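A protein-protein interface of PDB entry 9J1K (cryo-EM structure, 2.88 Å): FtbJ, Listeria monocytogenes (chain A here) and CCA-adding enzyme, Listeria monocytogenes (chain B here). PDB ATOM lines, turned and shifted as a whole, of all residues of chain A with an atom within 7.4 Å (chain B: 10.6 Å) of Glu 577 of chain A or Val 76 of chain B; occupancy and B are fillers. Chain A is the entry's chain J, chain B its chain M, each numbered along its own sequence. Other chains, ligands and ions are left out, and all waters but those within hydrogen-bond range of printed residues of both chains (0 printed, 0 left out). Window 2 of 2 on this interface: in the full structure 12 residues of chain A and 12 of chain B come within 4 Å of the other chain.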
ATOM      1  N   LEU A 573     -19.990  16.755  -0.408  1.00  0.00           N
ATOM      2  CA  LEU A 573     -18.690  17.304  -0.042  1.00  0.00           C
ATOM      3  C   LEU A 573     -18.506  17.307   1.472  1.00  0.00           C
ATOM      4  O   LEU A 573     -17.410  17.557   1.973  1.00  0.00           O
ATOM      5  CB  LEU A 573     -18.533  18.723  -0.592  1.00  0.00           C
ATOM      6  CG  LEU A 573     -17.762  18.867  -1.906  1.00  0.00           C
ATOM      7  CD1 LEU A 573     -16.369  18.265  -1.783  1.00  0.00           C
ATOM      8  CD2 LEU A 573     -18.531  18.231  -3.056  1.00  0.00           C
ATOM      9  N   ALA A 574     -19.595  17.035   2.194  1.00  0.00           N
ATOM     10  CA  ALA A 574     -19.545  17.041   3.653  1.00  0.00           C
ATOM     11  C   ALA A 574     -18.640  15.936   4.185  1.00  0.00           C
ATOM     12  O   ALA A 574     -17.898  16.147   5.150  1.00  0.00           O
ATOM     13  CB  ALA A 574     -20.954  16.909   4.228  1.00  0.00           C
ATOM     14  N   ARG A 575     -18.696  14.746   3.577  1.00  0.00           N
ATOM     15  CA  ARG A 575     -17.841  13.648   4.022  1.00  0.00           C
ATOM     16  C   ARG A 575     -16.379  13.910   3.695  1.00  0.00           C
ATOM     17  O   ARG A 575     -15.492  13.446   4.420  1.00  0.00           O
ATOM     18  CB  ARG A 575     -18.347  12.319   3.436  1.00  0.00           C
ATOM     19  CG  ARG A 575     -17.526  11.066   3.791  1.00  0.00           C
ATOM     20  CD  ARG A 575     -17.268  10.098   2.608  1.00  0.00           C
ATOM     21  NE  ARG A 575     -17.009  10.650   1.280  1.00  0.00           N
ATOM     22  CZ  ARG A 575     -16.111  11.576   0.974  1.00  0.00           C
ATOM     23  NH1 ARG A 575     -15.200  11.974   1.844  1.00  0.00           N
ATOM     24  NH2 ARG A 575     -16.090  12.070  -0.260  1.00  0.00           N
ATOM     25  N   VAL A 576     -16.108  14.673   2.636  1.00  0.00           N
ATOM     26  CA  VAL A 576     -14.745  15.135   2.385  1.00  0.00           C
ATOM     27  C   VAL A 576     -14.264  15.990   3.549  1.00  0.00           C
ATOM     28  O   VAL A 576     -13.143  15.824   4.047  1.00  0.00           O
ATOM     29  CB  VAL A 576     -14.681  15.902   1.053  1.00  0.00           C
ATOM     30  CG1 VAL A 576     -13.448  16.774   0.998  1.00  0.00           C
ATOM     31  CG2 VAL A 576     -14.695  14.938  -0.112  1.00  0.00           C
ATOM     32  N   GLU A 577     -15.114  16.908   4.013  1.00  0.00           N
ATOM     33  CA  GLU A 577     -14.760  17.740   5.160  1.00  0.00           C
ATOM     34  C   GLU A 577     -14.563  16.897   6.412  1.00  0.00           C
ATOM     35  O   GLU A 577     -13.640  17.145   7.195  1.00  0.00           O
ATOM     36  CB  GLU A 577     -15.839  18.795   5.392  1.00  0.00           C
ATOM     37  CG  GLU A 577     -16.170  19.617   4.162  1.00  0.00           C
ATOM     38  CD  GLU A 577     -14.936  20.004   3.376  1.00  0.00           C
ATOM     39  OE1 GLU A 577     -14.222  20.930   3.807  1.00  0.00           O
ATOM     40  OE2 GLU A 577     -14.681  19.384   2.323  1.00  0.00           O
ATOM     41  N   ASN A 578     -15.431  15.907   6.624  1.00  0.00           N
ATOM     42  CA  ASN A 578     -15.307  15.047   7.798  1.00  0.00           C
ATOM     43  C   ASN A 578     -13.994  14.276   7.773  1.00  0.00           C
ATOM     44  O   ASN A 578     -13.304  14.167   8.794  1.00  0.00           O
ATOM     45  CB  ASN A 578     -16.493  14.085   7.872  1.00  0.00           C
ATOM     46  CG  ASN A 578     -16.161  12.802   8.616  1.00  0.00           C
ATOM     47  OD1 ASN A 578     -15.713  12.831   9.764  1.00  0.00           O
ATOM     48  ND2 ASN A 578     -16.369  11.668   7.959  1.00  0.00           N
ATOM     49  N   LEU A 579     -13.631  13.732   6.609  1.00  0.00           N
ATOM     50  CA  LEU A 579     -12.387  12.979   6.509  1.00  0.00           C
ATOM     51  C   LEU A 579     -11.183  13.898   6.667  1.00  0.00           C
ATOM     52  O   LEU A 579     -10.178  13.510   7.269  1.00  0.00           O
ATOM     53  CB  LEU A 579     -12.338  12.211   5.182  1.00  0.00           C
ATOM     54  CG  LEU A 579     -11.035  11.611   4.630  1.00  0.00           C
ATOM     55  CD1 LEU A 579     -11.366  10.477   3.674  1.00  0.00           C
ATOM     56  CD2 LEU A 579     -10.162  12.624   3.906  1.00  0.00           C
ATOM     57  N   LEU A 580     -11.268  15.122   6.139  1.00  0.00           N
ATOM     58  CA  LEU A 580     -10.176  16.074   6.317  1.00  0.00           C
ATOM     59  C   LEU A 580     -10.012  16.463   7.780  1.00  0.00           C
ATOM     60  O   LEU A 580      -8.889  16.614   8.267  1.00  0.00           O
ATOM     61  CB  LEU A 580     -10.402  17.317   5.458  1.00  0.00           C
ATOM     62  CG  LEU A 580      -9.798  17.360   4.050  1.00  0.00           C
ATOM     63  CD1 LEU A 580      -8.309  17.687   4.110  1.00  0.00           C
ATOM     64  CD2 LEU A 580     -10.039  16.082   3.268  1.00  0.00           C
ATOM     65  N   GLU A 581     -11.122  16.633   8.501  1.00  0.00           N
ATOM     66  CA  GLU A 581     -11.036  16.929   9.929  1.00  0.00           C
ATOM     67  C   GLU A 581     -10.417  15.748  10.675  1.00  0.00           C
ATOM     68  O   GLU A 581      -9.468  15.920  11.455  1.00  0.00           O
ATOM     69  CB  GLU A 581     -12.440  17.262  10.450  1.00  0.00           C
ATOM     70  CG  GLU A 581     -12.692  17.392  11.966  1.00  0.00           C
ATOM     71  CD  GLU A 581     -11.481  17.789  12.792  1.00  0.00           C
ATOM     72  OE1 GLU A 581     -10.858  16.906  13.417  1.00  0.00           O
ATOM     73  OE2 GLU A 581     -11.162  18.996  12.826  1.00  0.00           O
ATOM     74  N   ARG A 582     -10.905  14.532  10.400  1.00  0.00           N
ATOM     75  CA  ARG A 582     -10.360  13.340  11.046  1.00  0.00           C
ATOM     76  C   ARG A 582      -8.873  13.190  10.754  1.00  0.00           C
ATOM     77  O   ARG A 582      -8.108  12.709  11.597  1.00  0.00           O
ATOM     78  CB  ARG A 582     -11.108  12.092  10.575  1.00  0.00           C
ATOM     79  CG  ARG A 582     -12.438  11.807  11.265  1.00  0.00           C
ATOM     80  CD  ARG A 582     -12.984  10.475  10.763  1.00  0.00           C
ATOM     81  NE  ARG A 582     -14.440  10.396  10.776  1.00  0.00           N
ATOM     82  CZ  ARG A 582     -15.142   9.508  10.084  1.00  0.00           C
ATOM     83  NH1 ARG A 582     -14.553   8.619   9.302  1.00  0.00           N
ATOM     84  NH2 ARG A 582     -16.469   9.517  10.173  1.00  0.00           N
ATOM     85  N   LEU A 583      -8.451  13.588   9.559  1.00  0.00           N
ATOM     86  CA  LEU A 583      -7.054  13.561   9.164  1.00  0.00           C
ATOM     87  C   LEU A 583      -6.259  14.727   9.730  1.00  0.00           C
ATOM     88  O   LEU A 583      -5.029  14.661   9.768  1.00  0.00           O
ATOM     89  CB  LEU A 583      -6.988  13.557   7.641  1.00  0.00           C
ATOM     90  CG  LEU A 583      -5.710  13.136   6.938  1.00  0.00           C
ATOM     91  CD1 LEU A 583      -5.441  11.684   7.201  1.00  0.00           C
ATOM     92  CD2 LEU A 583      -5.973  13.324   5.466  1.00  0.00           C
ATOM     93  N   ALA B  73     -17.401  25.144   0.426  1.00  0.00           N
ATOM     94  CA  ALA B  73     -16.157  25.575  -0.202  1.00  0.00           C
ATOM     95  C   ALA B  73     -15.344  26.453   0.744  1.00  0.00           C
ATOM     96  O   ALA B  73     -14.117  26.363   0.786  1.00  0.00           O
ATOM     97  CB  ALA B  73     -16.447  26.316  -1.497  1.00  0.00           C
ATOM     98  N   ILE B  74     -16.035  27.312   1.496  1.00  0.00           N
ATOM     99  CA  ILE B  74     -15.350  28.166   2.461  1.00  0.00           C
ATOM    100  C   ILE B  74     -14.794  27.335   3.613  1.00  0.00           C
ATOM    101  O   ILE B  74     -13.702  27.611   4.131  1.00  0.00           O
ATOM    102  CB  ILE B  74     -16.291  29.302   2.925  1.00  0.00           C
ATOM    103  CG1 ILE B  74     -17.415  28.837   3.872  1.00  0.00           C
ATOM    104  CG2 ILE B  74     -16.893  30.013   1.719  1.00  0.00           C
ATOM    105  CD1 ILE B  74     -17.052  28.723   5.354  1.00  0.00           C
ATOM    106  N   LEU B  75     -15.523  26.293   4.022  1.00  0.00           N
ATOM    107  CA  LEU B  75     -15.028  25.463   5.110  1.00  0.00           C
ATOM    108  C   LEU B  75     -13.866  24.603   4.635  1.00  0.00           C
ATOM    109  O   LEU B  75     -13.036  24.188   5.446  1.00  0.00           O
ATOM    110  CB  LEU B  75     -16.175  24.627   5.695  1.00  0.00           C
ATOM    111  CG  LEU B  75     -15.984  23.582   6.807  1.00  0.00           C
ATOM    112  CD1 LEU B  75     -15.370  22.272   6.352  1.00  0.00           C
ATOM    113  CD2 LEU B  75     -15.161  24.182   7.945  1.00  0.00           C
ATOM    114  N   VAL B  76     -13.763  24.367   3.325  1.00  0.00           N
ATOM    115  CA  VAL B  76     -12.551  23.769   2.771  1.00  0.00           C
ATOM    116  C   VAL B  76     -11.354  24.676   3.033  1.00  0.00           C
ATOM    117  O   VAL B  76     -10.278  24.214   3.432  1.00  0.00           O
ATOM    118  CB  VAL B  76     -12.729  23.483   1.267  1.00  0.00           C
ATOM    119  CG1 VAL B  76     -11.416  23.665   0.515  1.00  0.00           C
ATOM    120  CG2 VAL B  76     -13.276  22.085   1.044  1.00  0.00           C
ATOM    121  N   SER B  77     -11.527  25.983   2.816  1.00  0.00           N
ATOM    122  CA  SER B  77     -10.451  26.934   3.084  1.00  0.00           C
ATOM    123  C   SER B  77     -10.099  26.965   4.565  1.00  0.00           C
ATOM    124  O   SER B  77      -8.921  27.003   4.935  1.00  0.00           O
ATOM    125  CB  SER B  77     -10.850  28.326   2.600  1.00  0.00           C
ATOM    126  OG  SER B  77      -9.734  29.199   2.589  1.00  0.00           O
ATOM    127  N   GLU B  78     -11.117  26.968   5.432  1.00  0.00           N
ATOM    128  CA  GLU B  78     -10.852  26.955   6.869  1.00  0.00           C
ATOM    129  C   GLU B  78     -10.117  25.683   7.281  1.00  0.00           C
ATOM    130  O   GLU B  78      -9.193  25.723   8.107  1.00  0.00           O
ATOM    131  CB  GLU B  78     -12.160  27.097   7.645  1.00  0.00           C
ATOM    132  CG  GLU B  78     -11.974  27.474   9.105  1.00  0.00           C
ATOM    133  CD  GLU B  78     -12.094  26.282  10.035  1.00  0.00           C
ATOM    134  OE1 GLU B  78     -12.009  25.133   9.553  1.00  0.00           O
ATOM    135  OE2 GLU B  78     -12.268  26.495  11.254  1.00  0.00           O
ATOM    136  N   ASN B  79     -10.523  24.544   6.716  1.00  0.00           N
ATOM    137  CA  ASN B  79      -9.861  23.280   7.007  1.00  0.00           C
ATOM    138  C   ASN B  79      -8.409  23.309   6.560  1.00  0.00           C
ATOM    139  O   ASN B  79      -7.524  22.848   7.281  1.00  0.00           O
ATOM    140  CB  ASN B  79     -10.607  22.132   6.327  1.00  0.00           C
ATOM    141  CG  ASN B  79      -9.978  20.788   6.612  1.00  0.00           C
ATOM    142  OD1 ASN B  79      -9.316  20.212   5.752  1.00  0.00           O
ATOM    143  ND2 ASN B  79     -10.185  20.278   7.820  1.00  0.00           N
ATOM    144  N   GLY B  80      -8.143  23.847   5.368  1.00  0.00           N
ATOM    145  CA  GLY B  80      -6.766  23.958   4.912  1.00  0.00           C
ATOM    146  C   GLY B  80      -5.936  24.878   5.786  1.00  0.00           C
ATOM    147  O   GLY B  80      -4.767  24.594   6.078  1.00  0.00           O
ATOM    148  N   SER B  81      -6.528  25.993   6.220  1.00  0.00           N
ATOM    149  CA  SER B  81      -5.824  26.920   7.099  1.00  0.00           C
ATOM    150  C   SER B  81      -5.430  26.242   8.405  1.00  0.00           C
ATOM    151  O   SER B  81      -4.262  26.278   8.809  1.00  0.00           O
ATOM    152  CB  SER B  81      -6.695  28.148   7.371  1.00  0.00           C
ATOM    153  OG  SER B  81      -7.799  27.821   8.198  1.00  0.00           O
ATOM    154  N   ASN B  82      -6.395  25.606   9.075  1.00  0.00           N
ATOM    155  CA  ASN B  82      -6.079  24.918  10.324  1.00  0.00           C
ATOM    156  C   ASN B  82      -5.137  23.746  10.083  1.00  0.00           C
ATOM    157  O   ASN B  82      -4.277  23.447  10.920  1.00  0.00           O
ATOM    158  CB  ASN B  82      -7.361  24.452  11.009  1.00  0.00           C
ATOM    159  CG  ASN B  82      -7.739  25.326  12.187  1.00  0.00           C
ATOM    160  OD1 ASN B  82      -7.357  26.494  12.253  1.00  0.00           O
ATOM    161  ND2 ASN B  82      -8.491  24.764  13.127  1.00  0.00           N
ATOM    162  N   PHE B  83      -5.273  23.088   8.930  1.00  0.00           N
ATOM    163  CA  PHE B  83      -4.412  21.981   8.542  1.00  0.00           C
ATOM    164  C   PHE B  83      -2.953  22.410   8.551  1.00  0.00           C
ATOM    165  O   PHE B  83      -2.111  21.831   9.249  1.00  0.00           O
ATOM    166  CB  PHE B  83      -4.828  21.529   7.139  1.00  0.00           C
ATOM    167  CG  PHE B  83      -4.886  20.045   6.948  1.00  0.00           C
ATOM    168  CD1 PHE B  83      -4.226  19.447   5.890  1.00  0.00           C
ATOM    169  CD2 PHE B  83      -5.647  19.256   7.789  1.00  0.00           C
ATOM    170  CE1 PHE B  83      -4.299  18.087   5.694  1.00  0.00           C
ATOM    171  CE2 PHE B  83      -5.718  17.892   7.597  1.00  0.00           C
ATOM    172  CZ  PHE B  83      -5.042  17.306   6.551  1.00  0.00           C
ATOM    173  N   LYS B  84      -2.654  23.473   7.806  1.00  0.00           N
ATOM    174  CA  LYS B  84      -1.271  23.913   7.681  1.00  0.00           C
ATOM    175  C   LYS B  84      -0.779  24.576   8.964  1.00  0.00           C
ATOM    176  O   LYS B  84       0.402  24.445   9.315  1.00  0.00           O
ATOM    177  CB  LYS B  84      -1.144  24.850   6.481  1.00  0.00           C
ATOM    178  CG  LYS B  84      -0.827  24.128   5.180  1.00  0.00           C
ATOM    179  CD  LYS B  84      -0.569  25.093   4.033  1.00  0.00           C
ATOM    180  CE  LYS B  84       0.500  26.108   4.374  1.00  0.00           C
ATOM    181  NZ  LYS B  84       1.541  26.188   3.316  1.00  0.00           N
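Among the printed residues, pairs that only touch across the chains: Glu 577 of chain A with Leu 75 of chain B, Leu 580 of chain A with Asn 79 of chain B, Glu 577 of chain A with Val 76 of chain B, Leu 580 of chain A with Phe 83 of chain B, Glu 581 of chain A with Asn 79 of chain B and Leu 583 of chain A with Phe 83 of chain B.
Of chain B, only Leu 75 and Val 76 come within 4 Å of Glu 577 of chain A.
Of chain A, only Glu 577 comes within 4 Å of Val 76 of chain B.
No residue of chain B comes within 4 Å of Val 576 of chain A.
No residue of chain B comes within 4 Å of Asn 578 of chain A.
Of the printed residues of chain A, Phe 83 of chain B touches Leu 580 (3.5 Å) and Leu 583 (3.9 Å).
Printed residues of chain A within 4 Å of Leu 75 of chain B: Glu 577 (3.1 Å).
Of the printed residues of chain A, Asn 79 of chain B touches Leu 580 (3.1 Å) and Glu 581 (3.8 Å).
Of the printed residues of chain B, Glu 581 of chain A touches Asn 79.
Of the printed residues of chain B, Leu 583 of chain A touches Phe 83.
Arg 575 of chain A touches none of the printed residues of chain B.
The nearest residue of chain B that does not touch Glu 577 of chain A is Asn 79 of chain B (4.6 Å).
The nearest printed residue of chain B that does not touch Glu 581 of chain A is Phe 83 of chain B (5.6 Å).
Among the printed residues, 6 pairs touch across the chains.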
